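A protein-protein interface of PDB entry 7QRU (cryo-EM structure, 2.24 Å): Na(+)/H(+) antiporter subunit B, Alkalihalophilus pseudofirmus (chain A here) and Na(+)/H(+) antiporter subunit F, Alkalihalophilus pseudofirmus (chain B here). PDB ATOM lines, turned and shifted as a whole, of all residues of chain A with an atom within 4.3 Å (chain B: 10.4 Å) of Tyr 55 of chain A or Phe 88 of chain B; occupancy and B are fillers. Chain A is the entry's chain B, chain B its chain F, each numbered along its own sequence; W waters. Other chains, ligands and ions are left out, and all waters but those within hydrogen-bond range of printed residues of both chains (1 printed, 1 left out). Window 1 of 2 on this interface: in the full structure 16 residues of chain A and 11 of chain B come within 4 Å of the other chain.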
ATOM      1  N   LEU A  51     -13.363  17.829   0.611  1.00  0.00           N
ATOM      2  CA  LEU A  51     -14.431  16.898   0.927  1.00  0.00           C
ATOM      3  C   LEU A  51     -13.865  15.804   1.796  1.00  0.00           C
ATOM      4  O   LEU A  51     -14.515  15.425   2.734  1.00  0.00           O
ATOM      5  CB  LEU A  51     -15.126  16.335  -0.317  1.00  0.00           C
ATOM      6  CG  LEU A  51     -15.543  17.373  -1.342  1.00  0.00           C
ATOM      7  CD1 LEU A  51     -16.132  16.715  -2.540  1.00  0.00           C
ATOM      8  CD2 LEU A  51     -16.500  18.428  -0.784  1.00  0.00           C
ATOM      9  N   LEU A  52     -12.644  15.355   1.598  1.00  0.00           N
ATOM     10  CA  LEU A  52     -12.077  14.333   2.458  1.00  0.00           C
ATOM     11  C   LEU A  52     -11.990  14.849   3.877  1.00  0.00           C
ATOM     12  O   LEU A  52     -12.263  14.058   4.789  1.00  0.00           O
ATOM     13  CB  LEU A  52     -10.692  13.926   1.928  1.00  0.00           C
ATOM     14  CG  LEU A  52     -10.811  13.228   0.560  1.00  0.00           C
ATOM     15  CD1 LEU A  52      -9.439  13.052  -0.138  1.00  0.00           C
ATOM     16  CD2 LEU A  52     -11.561  11.903   0.711  1.00  0.00           C
ATOM     17  N   LEU A  53     -11.537  16.118   4.096  1.00  0.00           N
ATOM     18  CA  LEU A  53     -11.460  16.583   5.467  1.00  0.00           C
ATOM     19  C   LEU A  53     -12.832  16.537   6.166  1.00  0.00           C
ATOM     20  O   LEU A  53     -12.870  16.112   7.316  1.00  0.00           O
ATOM     21  CB  LEU A  53     -10.866  17.969   5.446  1.00  0.00           C
ATOM     22  CG  LEU A  53     -10.867  18.643   6.815  1.00  0.00           C
ATOM     23  CD1 LEU A  53     -10.053  17.816   7.793  1.00  0.00           C
ATOM     24  CD2 LEU A  53     -10.323  20.031   6.656  1.00  0.00           C
ATOM     25  N   MET A  54     -13.956  16.820   5.457  1.00  0.00           N
ATOM     26  CA  MET A  54     -15.306  16.640   5.975  1.00  0.00           C
ATOM     27  C   MET A  54     -15.547  15.184   6.358  1.00  0.00           C
ATOM     28  O   MET A  54     -15.959  14.920   7.412  1.00  0.00           O
ATOM     29  CB  MET A  54     -16.374  17.050   4.939  1.00  0.00           C
ATOM     30  CG  MET A  54     -16.517  18.510   4.745  1.00  0.00           C
ATOM     31  SD  MET A  54     -17.432  18.963   3.209  1.00  0.00           S
ATOM     32  CE  MET A  54     -19.096  18.699   3.782  1.00  0.00           C
ATOM     33  N   TYR A  55     -15.175  14.195   5.552  1.00  0.00           N
ATOM     34  CA  TYR A  55     -15.301  12.767   5.908  1.00  0.00           C
ATOM     35  C   TYR A  55     -14.426  12.414   7.109  1.00  0.00           C
ATOM     36  O   TYR A  55     -14.882  11.878   8.103  1.00  0.00           O
ATOM     37  CB  TYR A  55     -15.033  11.878   4.694  1.00  0.00           C
ATOM     38  CG  TYR A  55     -16.222  11.710   3.792  1.00  0.00           C
ATOM     39  CD1 TYR A  55     -17.257  10.878   4.156  1.00  0.00           C
ATOM     40  CD2 TYR A  55     -16.312  12.379   2.571  1.00  0.00           C
ATOM     41  CE1 TYR A  55     -18.332  10.651   3.305  1.00  0.00           C
ATOM     42  CE2 TYR A  55     -17.387  12.196   1.708  1.00  0.00           C
ATOM     43  CZ  TYR A  55     -18.400  11.333   2.076  1.00  0.00           C
ATOM     44  OH  TYR A  55     -19.486  11.231   1.210  1.00  0.00           O
ATOM     45  N   LEU A  56     -13.212  12.910   7.142  1.00  0.00           N
ATOM     46  CA  LEU A  56     -12.332  12.693   8.285  1.00  0.00           C
ATOM     47  C   LEU A  56     -12.866  13.277   9.587  1.00  0.00           C
ATOM     48  O   LEU A  56     -12.566  12.790  10.639  1.00  0.00           O
ATOM     49  CB  LEU A  56     -11.057  13.436   7.921  1.00  0.00           C
ATOM     50  CG  LEU A  56      -9.743  12.777   8.224  1.00  0.00           C
ATOM     51  CD1 LEU A  56      -9.744  11.376   7.738  1.00  0.00           C
ATOM     52  CD2 LEU A  56      -8.649  13.567   7.517  1.00  0.00           C
ATOM     53  N   GLY A  57     -13.361  14.521   9.508  1.00  0.00           N
ATOM     54  CA  GLY A  57     -13.782  15.257  10.664  1.00  0.00           C
ATOM     55  C   GLY A  57     -15.103  14.750  11.222  1.00  0.00           C
ATOM     56  O   GLY A  57     -15.375  15.026  12.392  1.00  0.00           O
ATOM     57  N   PHE A  58     -15.985  14.191  10.362  1.00  0.00           N
ATOM     58  CA  PHE A  58     -17.306  13.828  10.798  1.00  0.00           C
ATOM     59  C   PHE A  58     -17.418  12.330  10.618  1.00  0.00           C
ATOM     60  O   PHE A  58     -16.652  11.632  11.267  1.00  0.00           O
ATOM     61  CB  PHE A  58     -18.334  14.734  10.115  1.00  0.00           C
ATOM     62  CG  PHE A  58     -18.357  16.153  10.552  1.00  0.00           C
ATOM     63  CD1 PHE A  58     -17.529  17.042   9.984  1.00  0.00           C
ATOM     64  CD2 PHE A  58     -19.159  16.613  11.579  1.00  0.00           C
ATOM     65  CE1 PHE A  58     -17.475  18.364  10.462  1.00  0.00           C
ATOM     66  CE2 PHE A  58     -19.146  17.960  11.981  1.00  0.00           C
ATOM     67  CZ  PHE A  58     -18.340  18.846  11.401  1.00  0.00           C
ATOM     68  N   ASP A  59     -18.432  11.810   9.931  1.00  0.00           N
ATOM     69  CA  ASP A  59     -18.530  10.369   9.668  1.00  0.00           C
ATOM     70  C   ASP A  59     -19.229  10.139   8.329  1.00  0.00           C
ATOM     71  O   ASP A  59     -19.666  11.109   7.710  1.00  0.00           O
ATOM     72  CB  ASP A  59     -19.242   9.599  10.774  1.00  0.00           C
ATOM     73  CG  ASP A  59     -20.642  10.057  11.151  1.00  0.00           C
ATOM     74  OD1 ASP A  59     -21.356  10.353  10.264  1.00  0.00           O
ATOM     75  OD2 ASP A  59     -21.013  10.056  12.385  1.00  0.00           O
ATOM     76  N   MET A  60     -19.183   8.916   7.765  1.00  0.00           N
ATOM     77  CA  MET A  60     -19.522   8.753   6.353  1.00  0.00           C
ATOM     78  C   MET A  60     -21.020   8.941   6.147  1.00  0.00           C
ATOM     79  O   MET A  60     -21.430   9.568   5.173  1.00  0.00           O
ATOM     80  CB  MET A  60     -19.065   7.420   5.821  1.00  0.00           C
ATOM     81  CG  MET A  60     -17.552   7.282   5.845  1.00  0.00           C
ATOM     82  SD  MET A  60     -16.997   5.790   5.018  1.00  0.00           S
ATOM     83  CE  MET A  60     -17.288   6.522   3.402  1.00  0.00           C
ATOM     84  N   ILE A  63     -21.952  12.794   6.122  1.00  0.00           N
ATOM     85  CA  ILE A  63     -21.389  13.626   5.144  1.00  0.00           C
ATOM     86  C   ILE A  63     -21.940  13.172   3.806  1.00  0.00           C
ATOM     87  O   ILE A  63     -22.174  13.994   2.935  1.00  0.00           O
ATOM     88  CB  ILE A  63     -19.857  13.518   5.199  1.00  0.00           C
ATOM     89  CG1 ILE A  63     -19.413  14.107   6.537  1.00  0.00           C
ATOM     90  CG2 ILE A  63     -19.206  14.215   3.927  1.00  0.00           C
ATOM     91  CD1 ILE A  63     -19.895  15.556   6.701  1.00  0.00           C
ATOM     92  N   LYS A  64     -22.245  11.880   3.656  1.00  0.00           N
ATOM     93  CA  LYS A  64     -22.898  11.459   2.427  1.00  0.00           C
ATOM     94  C   LYS A  64     -24.292  12.074   2.323  1.00  0.00           C
ATOM     95  O   LYS A  64     -24.688  12.410   1.229  1.00  0.00           O
ATOM     96  CB  LYS A  64     -22.916   9.939   2.368  1.00  0.00           C
ATOM     97  CG  LYS A  64     -23.387   9.301   1.088  1.00  0.00           C
ATOM     98  CD  LYS A  64     -22.663   7.974   0.870  1.00  0.00           C
ATOM     99  CE  LYS A  64     -23.032   7.311  -0.445  1.00  0.00           C
ATOM    100  NZ  LYS A  64     -24.501   7.195  -0.629  1.00  0.00           N
ATOM    101  N   ILE A  67     -23.450  16.071   1.291  1.00  0.00           N
ATOM    102  CA  ILE A  67     -22.845  16.309  -0.005  1.00  0.00           C
ATOM    103  C   ILE A  67     -23.062  15.044  -0.828  1.00  0.00           C
ATOM    104  O   ILE A  67     -22.189  14.180  -1.027  1.00  0.00           O
ATOM    105  CB  ILE A  67     -21.351  16.698   0.040  1.00  0.00           C
ATOM    106  CG1 ILE A  67     -20.505  15.624   0.719  1.00  0.00           C
ATOM    107  CG2 ILE A  67     -21.125  18.050   0.705  1.00  0.00           C
ATOM    108  CD1 ILE A  67     -18.996  15.753   0.492  1.00  0.00           C
ATOM    109  N   ILE A 136     -11.394   6.824  -2.847  1.00  0.00           N
ATOM    110  CA  ILE A 136     -11.252   6.774  -1.397  1.00  0.00           C
ATOM    111  C   ILE A 136     -12.512   6.269  -0.725  1.00  0.00           C
ATOM    112  O   ILE A 136     -12.420   5.393   0.129  1.00  0.00           O
ATOM    113  CB  ILE A 136     -10.830   8.148  -0.859  1.00  0.00           C
ATOM    114  CG1 ILE A 136      -9.331   8.284  -1.110  1.00  0.00           C
ATOM    115  CG2 ILE A 136     -11.159   8.298   0.620  1.00  0.00           C
ATOM    116  CD1 ILE A 136      -8.999   9.617  -1.367  1.00  0.00           C
ATOM    117  N   LEU A 137     -13.675   6.648  -1.247  1.00  0.00           N
ATOM    118  CA  LEU A 137     -14.894   6.207  -0.619  1.00  0.00           C
ATOM    119  C   LEU A 137     -15.195   4.740  -0.889  1.00  0.00           C
ATOM    120  O   LEU A 137     -15.922   4.150  -0.139  1.00  0.00           O
ATOM    121  CB  LEU A 137     -16.026   7.094  -1.120  1.00  0.00           C
ATOM    122  CG  LEU A 137     -16.041   8.538  -0.584  1.00  0.00           C
ATOM    123  CD1 LEU A 137     -17.370   9.168  -0.919  1.00  0.00           C
ATOM    124  CD2 LEU A 137     -15.818   8.611   0.884  1.00  0.00           C
ATOM    125  N   ALA A 140     -12.971   2.884   1.660  1.00  0.00           N
ATOM    126  CA  ALA A 140     -13.413   3.093   3.038  1.00  0.00           C
ATOM    127  C   ALA A 140     -14.717   2.344   3.323  1.00  0.00           C
ATOM    128  O   ALA A 140     -14.894   1.814   4.391  1.00  0.00           O
ATOM    129  CB  ALA A 140     -13.627   4.588   3.255  1.00  0.00           C
ATOM    130  N   ILE B  73      -4.428  17.745   7.515  1.00  0.00           N
ATOM    131  CA  ILE B  73      -5.163  16.540   7.118  1.00  0.00           C
ATOM    132  C   ILE B  73      -4.332  15.295   7.431  1.00  0.00           C
ATOM    133  O   ILE B  73      -4.813  14.341   7.985  1.00  0.00           O
ATOM    134  CB  ILE B  73      -5.558  16.598   5.627  1.00  0.00           C
ATOM    135  CG1 ILE B  73      -6.615  17.686   5.419  1.00  0.00           C
ATOM    136  CG2 ILE B  73      -6.052  15.257   5.078  1.00  0.00           C
ATOM    137  CD1 ILE B  73      -6.786  18.035   3.946  1.00  0.00           C
ATOM    138  N   ILE B  76      -4.484  14.604  11.481  1.00  0.00           N
ATOM    139  CA  ILE B  76      -5.794  14.148  11.917  1.00  0.00           C
ATOM    140  C   ILE B  76      -6.014  12.697  11.521  1.00  0.00           C
ATOM    141  O   ILE B  76      -6.299  11.870  12.389  1.00  0.00           O
ATOM    142  CB  ILE B  76      -6.905  15.023  11.348  1.00  0.00           C
ATOM    143  CG1 ILE B  76      -6.816  16.462  11.873  1.00  0.00           C
ATOM    144  CG2 ILE B  76      -8.261  14.427  11.625  1.00  0.00           C
ATOM    145  CD1 ILE B  76      -6.817  16.554  13.379  1.00  0.00           C
ATOM    146  N   ALA B  77      -5.687  12.354  10.271  1.00  0.00           N
ATOM    147  CA  ALA B  77      -5.805  11.001   9.792  1.00  0.00           C
ATOM    148  C   ALA B  77      -4.869  10.021  10.485  1.00  0.00           C
ATOM    149  O   ALA B  77      -5.317   8.965  10.955  1.00  0.00           O
ATOM    150  CB  ALA B  77      -5.559  10.970   8.335  1.00  0.00           C
ATOM    151  N   LEU B  78      -3.617  10.366  10.694  1.00  0.00           N
ATOM    152  CA  LEU B  78      -2.704   9.454  11.370  1.00  0.00           C
ATOM    153  C   LEU B  78      -3.027   9.351  12.849  1.00  0.00           C
ATOM    154  O   LEU B  78      -2.898   8.312  13.441  1.00  0.00           O
ATOM    155  CB  LEU B  78      -1.286   9.919  11.171  1.00  0.00           C
ATOM    156  CG  LEU B  78      -0.719   9.714   9.788  1.00  0.00           C
ATOM    157  CD1 LEU B  78       0.546  10.564   9.617  1.00  0.00           C
ATOM    158  CD2 LEU B  78      -0.379   8.296   9.634  1.00  0.00           C
ATOM    159  N   SER B  79      -3.507  10.371  13.470  1.00  0.00           N
ATOM    160  CA  SER B  79      -3.927  10.293  14.856  1.00  0.00           C
ATOM    161  C   SER B  79      -5.090   9.348  15.050  1.00  0.00           C
ATOM    162  O   SER B  79      -5.167   8.666  16.051  1.00  0.00           O
ATOM    163  CB  SER B  79      -4.404  11.678  15.319  1.00  0.00           C
ATOM    164  OG  SER B  79      -3.246  12.371  15.681  1.00  0.00           O
ATOM    165  N   LYS B  80      -6.059   9.393  14.140  1.00  0.00           N
ATOM    166  CA  LYS B  80      -7.209   8.532  14.231  1.00  0.00           C
ATOM    167  C   LYS B  80      -6.836   7.080  13.910  1.00  0.00           C
ATOM    168  O   LYS B  80      -7.282   6.166  14.558  1.00  0.00           O
ATOM    169  CB  LYS B  80      -8.282   8.950  13.235  1.00  0.00           C
ATOM    170  CG  LYS B  80      -8.887  10.298  13.428  1.00  0.00           C
ATOM    171  CD  LYS B  80     -10.049  10.527  12.471  1.00  0.00           C
ATOM    172  CE  LYS B  80     -11.094   9.434  12.580  1.00  0.00           C
ATOM    173  NZ  LYS B  80     -12.295   9.912  11.843  1.00  0.00           N
ATOM    174  N   PHE B  81      -5.971   6.889  12.906  1.00  0.00           N
ATOM    175  CA  PHE B  81      -5.524   5.555  12.590  1.00  0.00           C
ATOM    176  C   PHE B  81      -4.946   4.915  13.838  1.00  0.00           C
ATOM    177  O   PHE B  81      -5.179   3.736  14.085  1.00  0.00           O
ATOM    178  CB  PHE B  81      -4.520   5.571  11.412  1.00  0.00           C
ATOM    179  CG  PHE B  81      -4.320   4.193  10.867  1.00  0.00           C
ATOM    180  CD1 PHE B  81      -5.379   3.485  10.234  1.00  0.00           C
ATOM    181  CD2 PHE B  81      -3.165   3.517  11.251  1.00  0.00           C
ATOM    182  CE1 PHE B  81      -5.148   2.171   9.850  1.00  0.00           C
ATOM    183  CE2 PHE B  81      -3.009   2.171  10.936  1.00  0.00           C
ATOM    184  CZ  PHE B  81      -3.986   1.516  10.213  1.00  0.00           C
ATOM    185  N   ILE B  82      -3.992   5.607  14.478  1.00  0.00           N
ATOM    186  CA  ILE B  82      -3.294   5.087  15.634  1.00  0.00           C
ATOM    187  C   ILE B  82      -4.307   4.712  16.726  1.00  0.00           C
ATOM    188  O   ILE B  82      -4.147   3.671  17.341  1.00  0.00           O
ATOM    189  CB  ILE B  82      -2.265   6.104  16.108  1.00  0.00           C
ATOM    190  CG1 ILE B  82      -1.070   6.052  15.184  1.00  0.00           C
ATOM    191  CG2 ILE B  82      -1.833   5.983  17.561  1.00  0.00           C
ATOM    192  CD1 ILE B  82      -0.193   7.394  15.520  1.00  0.00           C
ATOM    193  N   ARG B  84      -7.829   4.246  16.515  1.00  0.00           N
ATOM    194  CA  ARG B  84      -8.982   3.426  16.164  1.00  0.00           C
ATOM    195  C   ARG B  84      -8.676   2.390  15.061  1.00  0.00           C
ATOM    196  O   ARG B  84      -9.376   1.372  15.005  1.00  0.00           O
ATOM    197  CB  ARG B  84     -10.110   4.333  15.660  1.00  0.00           C
ATOM    198  CG  ARG B  84     -11.039   4.759  16.764  1.00  0.00           C
ATOM    199  CD  ARG B  84     -11.993   5.852  16.306  1.00  0.00           C
ATOM    200  NE  ARG B  84     -11.323   7.119  16.516  1.00  0.00           N
ATOM    201  CZ  ARG B  84     -11.836   8.305  16.229  1.00  0.00           C
ATOM    202  NH1 ARG B  84     -13.089   8.395  15.815  1.00  0.00           N
ATOM    203  NH2 ARG B  84     -11.039   9.365  16.192  1.00  0.00           N
ATOM    204  N   GLY B  85      -7.680   2.635  14.217  1.00  0.00           N
ATOM    205  CA  GLY B  85      -7.396   1.760  13.130  1.00  0.00           C
ATOM    206  C   GLY B  85      -8.311   1.995  11.942  1.00  0.00           C
ATOM    207  O   GLY B  85      -8.165   1.256  10.989  1.00  0.00           O
ATOM    208  N   VAL B  86      -9.153   3.040  11.974  1.00  0.00           N
ATOM    209  CA  VAL B  86      -9.937   3.436  10.803  1.00  0.00           C
ATOM    210  C   VAL B  86      -9.694   4.923  10.555  1.00  0.00           C
ATOM    211  O   VAL B  86      -9.887   5.725  11.438  1.00  0.00           O
ATOM    212  CB  VAL B  86     -11.441   3.150  10.985  1.00  0.00           C
ATOM    213  CG1 VAL B  86     -11.793   1.709  10.719  1.00  0.00           C
ATOM    214  CG2 VAL B  86     -11.904   3.496  12.369  1.00  0.00           C
ATOM    215  N   VAL B  87      -9.339   5.381   9.368  1.00  0.00           N
ATOM    216  CA  VAL B  87      -9.391   6.814   9.034  1.00  0.00           C
ATOM    217  C   VAL B  87     -10.837   7.374   9.040  1.00  0.00           C
ATOM    218  O   VAL B  87     -11.056   8.460   9.534  1.00  0.00           O
ATOM    219  CB  VAL B  87      -8.728   7.068   7.665  1.00  0.00           C
ATOM    220  CG1 VAL B  87      -8.482   8.511   7.335  1.00  0.00           C
ATOM    221  CG2 VAL B  87      -7.344   6.435   7.725  1.00  0.00           C
ATOM    222  N   PHE B  88     -11.840   6.660   8.526  1.00  0.00           N
ATOM    223  CA  PHE B  88     -13.158   7.241   8.358  1.00  0.00           C
ATOM    224  C   PHE B  88     -14.172   6.475   9.174  1.00  0.00           C
ATOM    225  O   PHE B  88     -14.218   5.255   9.043  1.00  0.00           O
ATOM    226  CB  PHE B  88     -13.636   7.208   6.886  1.00  0.00           C
ATOM    227  CG  PHE B  88     -12.800   7.991   5.908  1.00  0.00           C
ATOM    228  CD1 PHE B  88     -12.658   9.386   5.931  1.00  0.00           C
ATOM    229  CD2 PHE B  88     -11.957   7.328   5.103  1.00  0.00           C
ATOM    230  CE1 PHE B  88     -11.874  10.078   5.025  1.00  0.00           C
ATOM    231  CE2 PHE B  88     -11.175   8.023   4.181  1.00  0.00           C
ATOM    232  CZ  PHE B  88     -11.130   9.397   4.142  1.00  0.00           C
ATOM    233  N   ASP B  89     -14.978   7.196   9.968  1.00  0.00           N
ATOM    234  CA  ASP B  89     -16.019   6.568  10.756  1.00  0.00           C
ATOM    235  C   ASP B  89     -17.280   6.232   9.938  1.00  0.00           C
ATOM    236  O   ASP B  89     -17.489   6.730   8.859  1.00  0.00           O
ATOM    237  CB  ASP B  89     -16.307   7.437  11.932  1.00  0.00           C
ATOM    238  CG  ASP B  89     -15.089   7.832  12.731  1.00  0.00           C
ATOM    239  OD1 ASP B  89     -14.161   7.003  12.825  1.00  0.00           O
ATOM    240  OD2 ASP B  89     -15.105   8.994  13.260  1.00  0.00           O
ATOM    241  N   ARG B  90     -18.014   5.247  10.441  1.00  0.00           N
ATOM    242  CA  ARG B  90     -19.302   4.728  10.022  1.00  0.00           C
ATOM    243  C   ARG B  90     -19.193   3.545   9.079  1.00  0.00           C
ATOM    244  O   ARG B  90     -20.205   2.847   8.973  1.00  0.00           O
ATOM    245  CB  ARG B  90     -20.283   5.795   9.513  1.00  0.00           C
ATOM    246  CG  ARG B  90     -20.833   6.601  10.697  1.00  0.00           C
ATOM    247  CD  ARG B  90     -21.500   5.745  11.721  1.00  0.00           C
ATOM    248  NE  ARG B  90     -21.792   6.482  12.951  1.00  0.00           N
ATOM    249  CZ  ARG B  90     -20.916   6.749  13.928  1.00  0.00           C
ATOM    250  NH1 ARG B  90     -19.719   6.189  13.924  1.00  0.00           N
ATOM    251  NH2 ARG B  90     -21.249   7.570  14.916  1.00  0.00           N
ATOM    252  N   GLY B  91     -18.055   3.314   8.409  1.00  0.00           N
ATOM    253  CA  GLY B  91     -18.085   2.653   7.096  1.00  0.00           C
ATOM    254  C   GLY B  91     -17.815   1.150   7.115  1.00  0.00           C
ATOM    255  O   GLY B  91     -17.332   0.687   8.173  1.00  0.00           O
ATOM    256  OXT GLY B  91     -18.080   0.489   6.060  1.00  0.00           O
HETATM  257  O   HOH W   1     -13.875   3.342   6.514  1.00  0.00           O
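O of Leu 56 of chain A lies within hydrogen-bond range of NZ of Lys 80 of chain B (3.1 Å). The side-chain carboxylate of Asp 59 of chain A lies within salt-bridge range of the guanidinium group of Arg 90 of chain B, at 3.6 Å. The backbone carbonyl oxygen of Asp 89 of chain B is in hydrogen-bond range of the backbone NH of Met 60 of chain A, 3.0 Å away.
NZ of Lys 80 of chain B is in hydrogen-bond range of O of Val 87 of chain B (3.0 Å). The side-chain amino group (NZ) of Lys 80 of chain B is in salt-bridge range of the side-chain carboxylate (OD2) of Asp 89 of chain B (3.3 Å). The guanidinium group (NH1) of Arg 84 of chain B lies within salt-bridge range of the side-chain carboxylate (OD2) of Asp 89 of chain B (3.3 Å).
Among the printed residues, merely in contact across the chains: Tyr 55 of chain A with Phe 88 of chain B, Leu 56 of chain A with Ile 73 of chain B, Leu 56 of chain A with Val 87 of chain B, Leu 56 of chain A with Phe 88 of chain B, Phe 58 of chain A with Asp 89 of chain B, Asp 59 of chain A with Asp 89 of chain B, Met 60 of chain A with Arg 90 of chain B, Met 60 of chain A with Gly 91 of chain B, Ile 136 of chain A with Phe 88 of chain B, Ala 140 of chain A with Phe 88 of chain B and Ala 140 of chain A with Gly 91 of chain B.
Of chain B, only Phe 88 comes within 4 Å of Tyr 55 of chain A. Of the printed residues of chain A, Phe 88 of chain B touches Tyr 55, Leu 56, Ile 136 and Ala 140. No residue of chain B comes within 4 Å of Met 54 of chain A. Met 60 of chain A touches three residues of chain B. No residue of chain B comes within 4 Å of Ile 63 of chain A. Ala 140 of chain A touches two residues of chain B. Printed residues of chain A within 4 Å of Gly 91 of chain B: Met 60 and Ala 140. Printed residues of chain A within 4 Å of Ile 73 of chain B: Leu 56 (3.9 Å). Of the printed residues of chain B, Ile 136 of chain A touches Phe 88 (3.6 Å). Lys 64 of chain A touches none of the printed residues of chain B. Ala 77 of chain B touches none of the printed residues of chain A. The nearest residue of chain B that does not touch Tyr 55 of chain A is Lys 80 of chain B (5.0 Å). The nearest printed residue of chain A that does not touch Phe 88 of chain B is Leu 52 of chain A (4.01 Å).
Of the 16 printed residues of chain B, 7 touch a printed residue of chain A. Hydrophobic or aromatic side chains of chain B within 4 Å of the printed part of chain A: Ile 73, Val 87 and Phe 88. Along chain B the printed residues that touch a printed residue of chain A span positions 73 to 91. Of the 16 printed residues of chain A, 7 touch a printed residue of chain B. Hydrophobic or aromatic side chains of chain A that line the printed part of chain B: Tyr 55, Leu 56, Met 60, Ile 136 and Ala 140. Among the printed residues, Asp or Glu carboxylates within 4 Å of a Lys or Arg side-chain nitrogen of the other chain: Asp 59 of chain A with Arg 90 of chain B.
Water W1 lies within hydrogen-bond range of the backbone carbonyl oxygen of Ala 140 of chain A (2.8 Å) and the backbone carbonyl oxygen of Phe 88 of chain B (3.2 Å).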
